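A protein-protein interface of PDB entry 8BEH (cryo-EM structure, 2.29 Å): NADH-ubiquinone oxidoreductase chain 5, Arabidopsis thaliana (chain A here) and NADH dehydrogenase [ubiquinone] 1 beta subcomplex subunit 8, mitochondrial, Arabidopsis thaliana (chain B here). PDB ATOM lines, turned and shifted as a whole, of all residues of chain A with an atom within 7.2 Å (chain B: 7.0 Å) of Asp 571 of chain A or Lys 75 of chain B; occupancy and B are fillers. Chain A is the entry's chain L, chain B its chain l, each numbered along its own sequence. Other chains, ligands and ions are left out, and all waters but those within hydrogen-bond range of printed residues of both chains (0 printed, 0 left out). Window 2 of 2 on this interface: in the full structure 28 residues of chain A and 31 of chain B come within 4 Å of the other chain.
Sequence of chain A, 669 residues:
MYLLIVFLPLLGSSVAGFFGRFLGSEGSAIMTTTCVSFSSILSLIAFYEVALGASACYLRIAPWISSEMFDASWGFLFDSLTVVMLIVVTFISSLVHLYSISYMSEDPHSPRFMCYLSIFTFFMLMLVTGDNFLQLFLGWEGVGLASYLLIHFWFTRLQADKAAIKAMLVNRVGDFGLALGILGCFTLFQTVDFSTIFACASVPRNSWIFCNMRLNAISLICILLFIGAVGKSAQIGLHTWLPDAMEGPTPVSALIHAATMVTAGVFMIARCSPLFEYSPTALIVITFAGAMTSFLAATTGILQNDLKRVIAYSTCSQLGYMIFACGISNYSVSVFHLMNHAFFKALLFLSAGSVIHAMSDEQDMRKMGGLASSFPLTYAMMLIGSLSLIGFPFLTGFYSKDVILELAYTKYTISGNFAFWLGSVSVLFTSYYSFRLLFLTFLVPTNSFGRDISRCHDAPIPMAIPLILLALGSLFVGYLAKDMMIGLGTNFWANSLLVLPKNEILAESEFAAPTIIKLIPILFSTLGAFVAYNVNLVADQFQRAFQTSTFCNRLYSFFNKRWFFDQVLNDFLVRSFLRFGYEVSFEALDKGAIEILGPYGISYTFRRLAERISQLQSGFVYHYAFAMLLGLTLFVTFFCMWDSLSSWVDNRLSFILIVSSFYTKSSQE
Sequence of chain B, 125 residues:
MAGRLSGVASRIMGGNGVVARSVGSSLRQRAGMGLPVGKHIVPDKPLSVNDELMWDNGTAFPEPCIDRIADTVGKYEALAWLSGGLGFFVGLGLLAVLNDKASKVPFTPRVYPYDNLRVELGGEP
OD1 of Asp 571 of chain A is in salt-bridge range of NH2 of Arg 575 of chain A (2.7 Å).
ND2 of Asn 570 of chain A is in hydrogen-bond range of OD1 of Asp 571 of chain A (3.3 Å).
The side-chain carboxylate of Glu 77 of chain B lies within hydrogen-bond range of the backbone NH of Gly 74 of chain B (3.3 Å).
The backbone carbonyl oxygen (O) of Phe 572 of chain A is in hydrogen-bond range of the side-chain hydroxyl (OG) of Ser 576 of chain A, at 3.0 Å.
O of Gly 74 of chain B is in hydrogen-bond range of NE2 of Gln 567 of chain A, 3.1 Å away.
NE2 of Gln 567 of chain A is in hydrogen-bond range of O of Val 73 of chain B, at 3.2 Å.
NZ of Lys 75 of chain B lies within hydrogen-bond range of O of Asp 571 of chain A, at 3.0 Å.
Printed residues of chain A that touch a printed residue of chain B: Phe 564, Gln 567, Val 568, Asp 571 and Phe 572.
Hydrophobic or aromatic side chains of chain A within 4 Å of the printed part of chain B: Phe 564, Val 568 and Phe 572.
Along chain A the printed residues that touch a printed residue of chain B span positions 564 to 572.
Hydrophobic or aromatic side chains of chain B that line the printed part of chain A: Val 73, Tyr 76, Ala 78 and Leu 79.
Among the printed residues, 12 pairs touch across the chains.
Among the printed residues, no Asp or Glu carboxylate lies within 4 Å of a Lys or Arg side-chain nitrogen of the other chain.
Asp 571 of chain A touches just one residue of chain B: Lys 75.
Of the printed residues of chain A, Lys 75 of chain B touches Asp 571 (3.0 Å) and Phe 572 (3.1 Å).
Printed residues of chain A within 4 Å of Tyr 76 of chain B: Phe 572 (3.8 Å).
Printed residues of chain A within 4 Å of Gly 74 of chain B: Gln 567.
Printed residues of chain B within 4 Å of Phe 564 of chain A: Val 73 (3.3 Å) and Ala 78 (3.8 Å).
Of the printed residues of chain A, Val 73 of chain B touches Phe 564 and Gln 567.
Of the printed residues of chain A, Ala 78 of chain B touches Phe 564, Gln 567 and Val 568.
The nearest residue of chain B that does not touch Asp 571 of chain A is Gly 74 of chain B (5.4 Å).
The nearest printed residue of chain B that does not touch Val 568 of chain A is Lys 75 of chain B (4.9 Å).
Phe 564 of chain A touches Val 73 of chain B.
CB of Phe 564 of chain A touches CB of Ala 78 of chain B, at 3.8 Å.
CA of Ala 70 of chain B touches OE1 of Gln 567 of chain A, at 3.3 Å.
CB of Ala 78 of chain B touches CD of Gln 567 of chain A, at 3.8 Å.
Val 568 of chain A touches Ala 78 of chain B (CG2 to O, 3.8 Å).
Val 568 of chain A touches Leu 79 of chain B (CG2 to N, 3.7 Å).
Lys 75 of chain B touches Phe 572 of chain A.
CE1 of Tyr 76 of chain B touches CE2 of Phe 572 of chain A (3.8 Å).
CD2 of Leu 79 of chain B touches CZ of Phe 572 of chain A (3.9 Å).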
ATOM      1  N   PHE A 564       5.003 -23.367 -19.282  1.00  0.00           N
ATOM      2  CA  PHE A 564       4.110 -23.967 -18.240  1.00  0.00           C
ATOM      3  C   PHE A 564       4.914 -24.222 -16.964  1.00  0.00           C
ATOM      4  O   PHE A 564       4.518 -25.046 -16.169  1.00  0.00           O
ATOM      5  CB  PHE A 564       3.321 -25.176 -18.786  1.00  0.00           C
ATOM      6  CG  PHE A 564       2.531 -25.026 -20.050  1.00  0.00           C
ATOM      7  CD1 PHE A 564       1.663 -23.967 -20.230  1.00  0.00           C
ATOM      8  CD2 PHE A 564       2.606 -26.001 -21.029  1.00  0.00           C
ATOM      9  CE1 PHE A 564       0.923 -23.858 -21.393  1.00  0.00           C
ATOM     10  CE2 PHE A 564       1.851 -25.901 -22.181  1.00  0.00           C
ATOM     11  CZ  PHE A 564       1.023 -24.826 -22.364  1.00  0.00           C
ATOM     12  N   PHE A 565       5.989 -23.478 -16.767  1.00  0.00           N
ATOM     13  CA  PHE A 565       6.867 -23.770 -15.640  1.00  0.00           C
ATOM     14  C   PHE A 565       6.181 -23.454 -14.315  1.00  0.00           C
ATOM     15  O   PHE A 565       6.195 -24.269 -13.385  1.00  0.00           O
ATOM     16  CB  PHE A 565       8.175 -22.995 -15.785  1.00  0.00           C
ATOM     17  CG  PHE A 565       9.349 -23.675 -15.153  1.00  0.00           C
ATOM     18  CD1 PHE A 565       9.513 -23.691 -13.782  1.00  0.00           C
ATOM     19  CD2 PHE A 565      10.281 -24.326 -15.940  1.00  0.00           C
ATOM     20  CE1 PHE A 565      10.600 -24.330 -13.212  1.00  0.00           C
ATOM     21  CE2 PHE A 565      11.362 -24.966 -15.377  1.00  0.00           C
ATOM     22  CZ  PHE A 565      11.522 -24.969 -14.015  1.00  0.00           C
ATOM     23  N   ASP A 566       5.562 -22.273 -14.220  1.00  0.00           N
ATOM     24  CA  ASP A 566       4.834 -21.911 -13.008  1.00  0.00           C
ATOM     25  C   ASP A 566       3.679 -22.864 -12.752  1.00  0.00           C
ATOM     26  O   ASP A 566       3.454 -23.282 -11.611  1.00  0.00           O
ATOM     27  CB  ASP A 566       4.317 -20.475 -13.100  1.00  0.00           C
ATOM     28  CG  ASP A 566       5.390 -19.452 -12.820  1.00  0.00           C
ATOM     29  OD1 ASP A 566       5.754 -19.289 -11.639  1.00  0.00           O
ATOM     30  OD2 ASP A 566       5.864 -18.804 -13.772  1.00  0.00           O
ATOM     31  N   GLN A 567       2.932 -23.213 -13.801  1.00  0.00           N
ATOM     32  CA  GLN A 567       1.825 -24.148 -13.646  1.00  0.00           C
ATOM     33  C   GLN A 567       2.304 -25.472 -13.071  1.00  0.00           C
ATOM     34  O   GLN A 567       1.740 -25.970 -12.094  1.00  0.00           O
ATOM     35  CB  GLN A 567       1.135 -24.379 -14.985  1.00  0.00           C
ATOM     36  CG  GLN A 567       0.226 -25.593 -14.992  1.00  0.00           C
ATOM     37  CD  GLN A 567      -0.897 -25.479 -15.993  1.00  0.00           C
ATOM     38  OE1 GLN A 567      -0.955 -24.535 -16.775  1.00  0.00           O
ATOM     39  NE2 GLN A 567      -1.812 -26.435 -15.959  1.00  0.00           N
ATOM     40  N   VAL A 568       3.342 -26.057 -13.671  1.00  0.00           N
ATOM     41  CA  VAL A 568       3.817 -27.365 -13.226  1.00  0.00           C
ATOM     42  C   VAL A 568       4.337 -27.287 -11.796  1.00  0.00           C
ATOM     43  O   VAL A 568       4.019 -28.141 -10.956  1.00  0.00           O
ATOM     44  CB  VAL A 568       4.884 -27.908 -14.195  1.00  0.00           C
ATOM     45  CG1 VAL A 568       5.639 -29.061 -13.565  1.00  0.00           C
ATOM     46  CG2 VAL A 568       4.231 -28.354 -15.492  1.00  0.00           C
ATOM     47  N   LEU A 569       5.134 -26.259 -11.490  1.00  0.00           N
ATOM     48  CA  LEU A 569       5.663 -26.134 -10.136  1.00  0.00           C
ATOM     49  C   LEU A 569       4.541 -25.993  -9.115  1.00  0.00           C
ATOM     50  O   LEU A 569       4.531 -26.689  -8.098  1.00  0.00           O
ATOM     51  CB  LEU A 569       6.634 -24.960 -10.035  1.00  0.00           C
ATOM     52  CG  LEU A 569       8.123 -25.293 -10.158  1.00  0.00           C
ATOM     53  CD1 LEU A 569       8.406 -26.271 -11.293  1.00  0.00           C
ATOM     54  CD2 LEU A 569       8.949 -24.022 -10.285  1.00  0.00           C
ATOM     55  N   ASN A 570       3.571 -25.121  -9.382  1.00  0.00           N
ATOM     56  CA  ASN A 570       2.479 -24.936  -8.434  1.00  0.00           C
ATOM     57  C   ASN A 570       1.633 -26.197  -8.301  1.00  0.00           C
ATOM     58  O   ASN A 570       1.212 -26.556  -7.196  1.00  0.00           O
ATOM     59  CB  ASN A 570       1.615 -23.752  -8.852  1.00  0.00           C
ATOM     60  CG  ASN A 570       0.363 -23.635  -8.024  1.00  0.00           C
ATOM     61  OD1 ASN A 570       0.382 -23.070  -6.934  1.00  0.00           O
ATOM     62  ND2 ASN A 570      -0.737 -24.175  -8.532  1.00  0.00           N
ATOM     63  N   ASP A 571       1.386 -26.891  -9.414  1.00  0.00           N
ATOM     64  CA  ASP A 571       0.509 -28.055  -9.392  1.00  0.00           C
ATOM     65  C   ASP A 571       1.138 -29.239  -8.679  1.00  0.00           C
ATOM     66  O   ASP A 571       0.427 -30.021  -8.044  1.00  0.00           O
ATOM     67  CB  ASP A 571       0.132 -28.462 -10.815  1.00  0.00           C
ATOM     68  CG  ASP A 571      -0.904 -27.552 -11.426  1.00  0.00           C
ATOM     69  OD1 ASP A 571      -1.152 -26.467 -10.860  1.00  0.00           O
ATOM     70  OD2 ASP A 571      -1.480 -27.927 -12.467  1.00  0.00           O
ATOM     71  N   PHE A 572       2.455 -29.404  -8.779  1.00  0.00           N
ATOM     72  CA  PHE A 572       3.069 -30.611  -8.254  1.00  0.00           C
ATOM     73  C   PHE A 572       3.904 -30.400  -7.000  1.00  0.00           C
ATOM     74  O   PHE A 572       4.174 -31.377  -6.297  1.00  0.00           O
ATOM     75  CB  PHE A 572       3.938 -31.276  -9.332  1.00  0.00           C
ATOM     76  CG  PHE A 572       3.149 -31.882 -10.458  1.00  0.00           C
ATOM     77  CD1 PHE A 572       2.773 -31.117 -11.550  1.00  0.00           C
ATOM     78  CD2 PHE A 572       2.787 -33.221 -10.430  1.00  0.00           C
ATOM     79  CE1 PHE A 572       2.053 -31.672 -12.590  1.00  0.00           C
ATOM     80  CE2 PHE A 572       2.066 -33.780 -11.466  1.00  0.00           C
ATOM     81  CZ  PHE A 572       1.696 -33.002 -12.549  1.00  0.00           C
ATOM     82  N   LEU A 573       4.298 -29.168  -6.683  1.00  0.00           N
ATOM     83  CA  LEU A 573       5.203 -28.902  -5.575  1.00  0.00           C
ATOM     84  C   LEU A 573       4.548 -28.050  -4.493  1.00  0.00           C
ATOM     85  O   LEU A 573       4.452 -28.487  -3.337  1.00  0.00           O
ATOM     86  CB  LEU A 573       6.453 -28.229  -6.167  1.00  0.00           C
ATOM     87  CG  LEU A 573       7.624 -27.638  -5.383  1.00  0.00           C
ATOM     88  CD1 LEU A 573       7.314 -26.272  -4.789  1.00  0.00           C
ATOM     89  CD2 LEU A 573       8.091 -28.601  -4.335  1.00  0.00           C
ATOM     90  N   VAL A 574       4.069 -26.854  -4.843  1.00  0.00           N
ATOM     91  CA  VAL A 574       3.478 -25.957  -3.853  1.00  0.00           C
ATOM     92  C   VAL A 574       2.189 -26.548  -3.300  1.00  0.00           C
ATOM     93  O   VAL A 574       1.957 -26.547  -2.086  1.00  0.00           O
ATOM     94  CB  VAL A 574       3.240 -24.563  -4.459  1.00  0.00           C
ATOM     95  CG1 VAL A 574       3.036 -23.543  -3.362  1.00  0.00           C
ATOM     96  CG2 VAL A 574       4.404 -24.161  -5.350  1.00  0.00           C
ATOM     97  N   ARG A 575       1.333 -27.057  -4.186  1.00  0.00           N
ATOM     98  CA  ARG A 575       0.115 -27.719  -3.743  1.00  0.00           C
ATOM     99  C   ARG A 575       0.429 -28.956  -2.913  1.00  0.00           C
ATOM    100  O   ARG A 575      -0.267 -29.240  -1.936  1.00  0.00           O
ATOM    101  CB  ARG A 575      -0.768 -28.068  -4.946  1.00  0.00           C
ATOM    102  CG  ARG A 575      -1.979 -28.918  -4.586  1.00  0.00           C
ATOM    103  CD  ARG A 575      -3.268 -28.579  -5.342  1.00  0.00           C
ATOM    104  NE  ARG A 575      -3.114 -27.738  -6.524  1.00  0.00           N
ATOM    105  CZ  ARG A 575      -2.628 -28.151  -7.687  1.00  0.00           C
ATOM    106  NH1 ARG A 575      -2.201 -29.391  -7.860  1.00  0.00           N
ATOM    107  NH2 ARG A 575      -2.582 -27.299  -8.707  1.00  0.00           N
ATOM    108  N   SER A 576       1.483 -29.692  -3.269  1.00  0.00           N
ATOM    109  CA  SER A 576       1.864 -30.864  -2.488  1.00  0.00           C
ATOM    110  C   SER A 576       2.201 -30.485  -1.051  1.00  0.00           C
ATOM    111  O   SER A 576       1.677 -31.079  -0.102  1.00  0.00           O
ATOM    112  CB  SER A 576       3.047 -31.576  -3.144  1.00  0.00           C
ATOM    113  OG  SER A 576       2.609 -32.575  -4.040  1.00  0.00           O
ATOM    114  N   ALA B  70      -2.649 -21.198 -16.929  1.00  0.00           N
ATOM    115  CA  ALA B  70      -3.062 -22.121 -15.879  1.00  0.00           C
ATOM    116  C   ALA B  70      -4.574 -22.318 -15.885  1.00  0.00           C
ATOM    117  O   ALA B  70      -5.153 -22.745 -14.886  1.00  0.00           O
ATOM    118  CB  ALA B  70      -2.599 -21.618 -14.520  1.00  0.00           C
ATOM    119  N   VAL B  73      -4.622 -24.918 -20.255  1.00  0.00           N
ATOM    120  CA  VAL B  73      -3.888 -26.207 -20.391  1.00  0.00           C
ATOM    121  C   VAL B  73      -4.088 -27.098 -19.150  1.00  0.00           C
ATOM    122  O   VAL B  73      -4.229 -26.561 -18.080  1.00  0.00           O
ATOM    123  CB  VAL B  73      -2.422 -25.910 -20.782  1.00  0.00           C
ATOM    124  CG1 VAL B  73      -1.753 -27.068 -21.500  1.00  0.00           C
ATOM    125  CG2 VAL B  73      -2.299 -24.629 -21.580  1.00  0.00           C
ATOM    126  N   GLY B  74      -4.178 -28.421 -19.307  1.00  0.00           N
ATOM    127  CA  GLY B  74      -4.322 -29.378 -18.230  1.00  0.00           C
ATOM    128  C   GLY B  74      -3.056 -29.514 -17.403  1.00  0.00           C
ATOM    129  O   GLY B  74      -1.995 -28.985 -17.727  1.00  0.00           O
ATOM    130  N   LYS B  75      -3.178 -30.251 -16.301  1.00  0.00           N
ATOM    131  CA  LYS B  75      -2.069 -30.390 -15.364  1.00  0.00           C
ATOM    132  C   LYS B  75      -0.998 -31.326 -15.920  1.00  0.00           C
ATOM    133  O   LYS B  75       0.161 -30.933 -16.112  1.00  0.00           O
ATOM    134  CB  LYS B  75      -2.612 -30.888 -14.022  1.00  0.00           C
ATOM    135  CG  LYS B  75      -1.682 -31.726 -13.167  1.00  0.00           C
ATOM    136  CD  LYS B  75      -2.129 -31.637 -11.720  1.00  0.00           C
ATOM    137  CE  LYS B  75      -1.346 -32.549 -10.803  1.00  0.00           C
ATOM    138  NZ  LYS B  75      -0.131 -31.877 -10.274  1.00  0.00           N
ATOM    139  N   TYR B  76      -1.378 -32.571 -16.209  1.00  0.00           N
ATOM    140  CA  TYR B  76      -0.417 -33.529 -16.735  1.00  0.00           C
ATOM    141  C   TYR B  76      -0.028 -33.201 -18.167  1.00  0.00           C
ATOM    142  O   TYR B  76       1.084 -33.523 -18.592  1.00  0.00           O
ATOM    143  CB  TYR B  76      -0.979 -34.945 -16.633  1.00  0.00           C
ATOM    144  CG  TYR B  76      -1.072 -35.438 -15.213  1.00  0.00           C
ATOM    145  CD1 TYR B  76       0.032 -35.987 -14.578  1.00  0.00           C
ATOM    146  CD2 TYR B  76      -2.256 -35.334 -14.498  1.00  0.00           C
ATOM    147  CE1 TYR B  76      -0.044 -36.431 -13.280  1.00  0.00           C
ATOM    148  CE2 TYR B  76      -2.339 -35.773 -13.199  1.00  0.00           C
ATOM    149  CZ  TYR B  76      -1.232 -36.321 -12.594  1.00  0.00           C
ATOM    150  OH  TYR B  76      -1.313 -36.765 -11.297  1.00  0.00           O
ATOM    151  N   GLU B  77      -0.928 -32.610 -18.918  1.00  0.00           N
ATOM    152  CA  GLU B  77      -0.579 -32.103 -20.269  1.00  0.00           C
ATOM    153  C   GLU B  77       0.497 -31.007 -20.181  1.00  0.00           C
ATOM    154  O   GLU B  77       1.381 -31.001 -20.993  1.00  0.00           O
ATOM    155  CB  GLU B  77      -1.830 -31.521 -20.893  1.00  0.00           C
ATOM    156  CG  GLU B  77      -1.650 -31.297 -22.378  1.00  0.00           C
ATOM    157  CD  GLU B  77      -2.464 -30.165 -22.954  1.00  0.00           C
ATOM    158  OE1 GLU B  77      -3.334 -29.646 -22.232  1.00  0.00           O
ATOM    159  OE2 GLU B  77      -2.234 -29.815 -24.125  1.00  0.00           O
ATOM    160  N   ALA B  78       0.346 -30.075 -19.266  1.00  0.00           N
ATOM    161  CA  ALA B  78       1.384 -29.070 -19.067  1.00  0.00           C
ATOM    162  C   ALA B  78       2.693 -29.719 -18.642  1.00  0.00           C
ATOM    163  O   ALA B  78       3.771 -29.312 -19.092  1.00  0.00           O
ATOM    164  CB  ALA B  78       0.935 -28.038 -18.034  1.00  0.00           C
ATOM    165  N   LEU B  79       2.618 -30.737 -17.780  1.00  0.00           N
ATOM    166  CA  LEU B  79       3.827 -31.465 -17.410  1.00  0.00           C
ATOM    167  C   LEU B  79       4.472 -32.116 -18.630  1.00  0.00           C
ATOM    168  O   LEU B  79       5.696 -32.090 -18.779  1.00  0.00           O
ATOM    169  CB  LEU B  79       3.510 -32.509 -16.341  1.00  0.00           C
ATOM    170  CG  LEU B  79       4.604 -33.521 -15.988  1.00  0.00           C
ATOM    171  CD1 LEU B  79       5.762 -32.852 -15.267  1.00  0.00           C
ATOM    172  CD2 LEU B  79       4.033 -34.638 -15.138  1.00  0.00           C
ATOM    173  N   ALA B  80       3.662 -32.696 -19.518  1.00  0.00           N
ATOM    174  CA  ALA B  80       4.197 -33.333 -20.719  1.00  0.00           C
ATOM    175  C   ALA B  80       4.850 -32.319 -21.654  1.00  0.00           C
ATOM    176  O   ALA B  80       5.926 -32.576 -22.206  1.00  0.00           O
ATOM    177  CB  ALA B  80       3.092 -34.099 -21.445  1.00  0.00           C
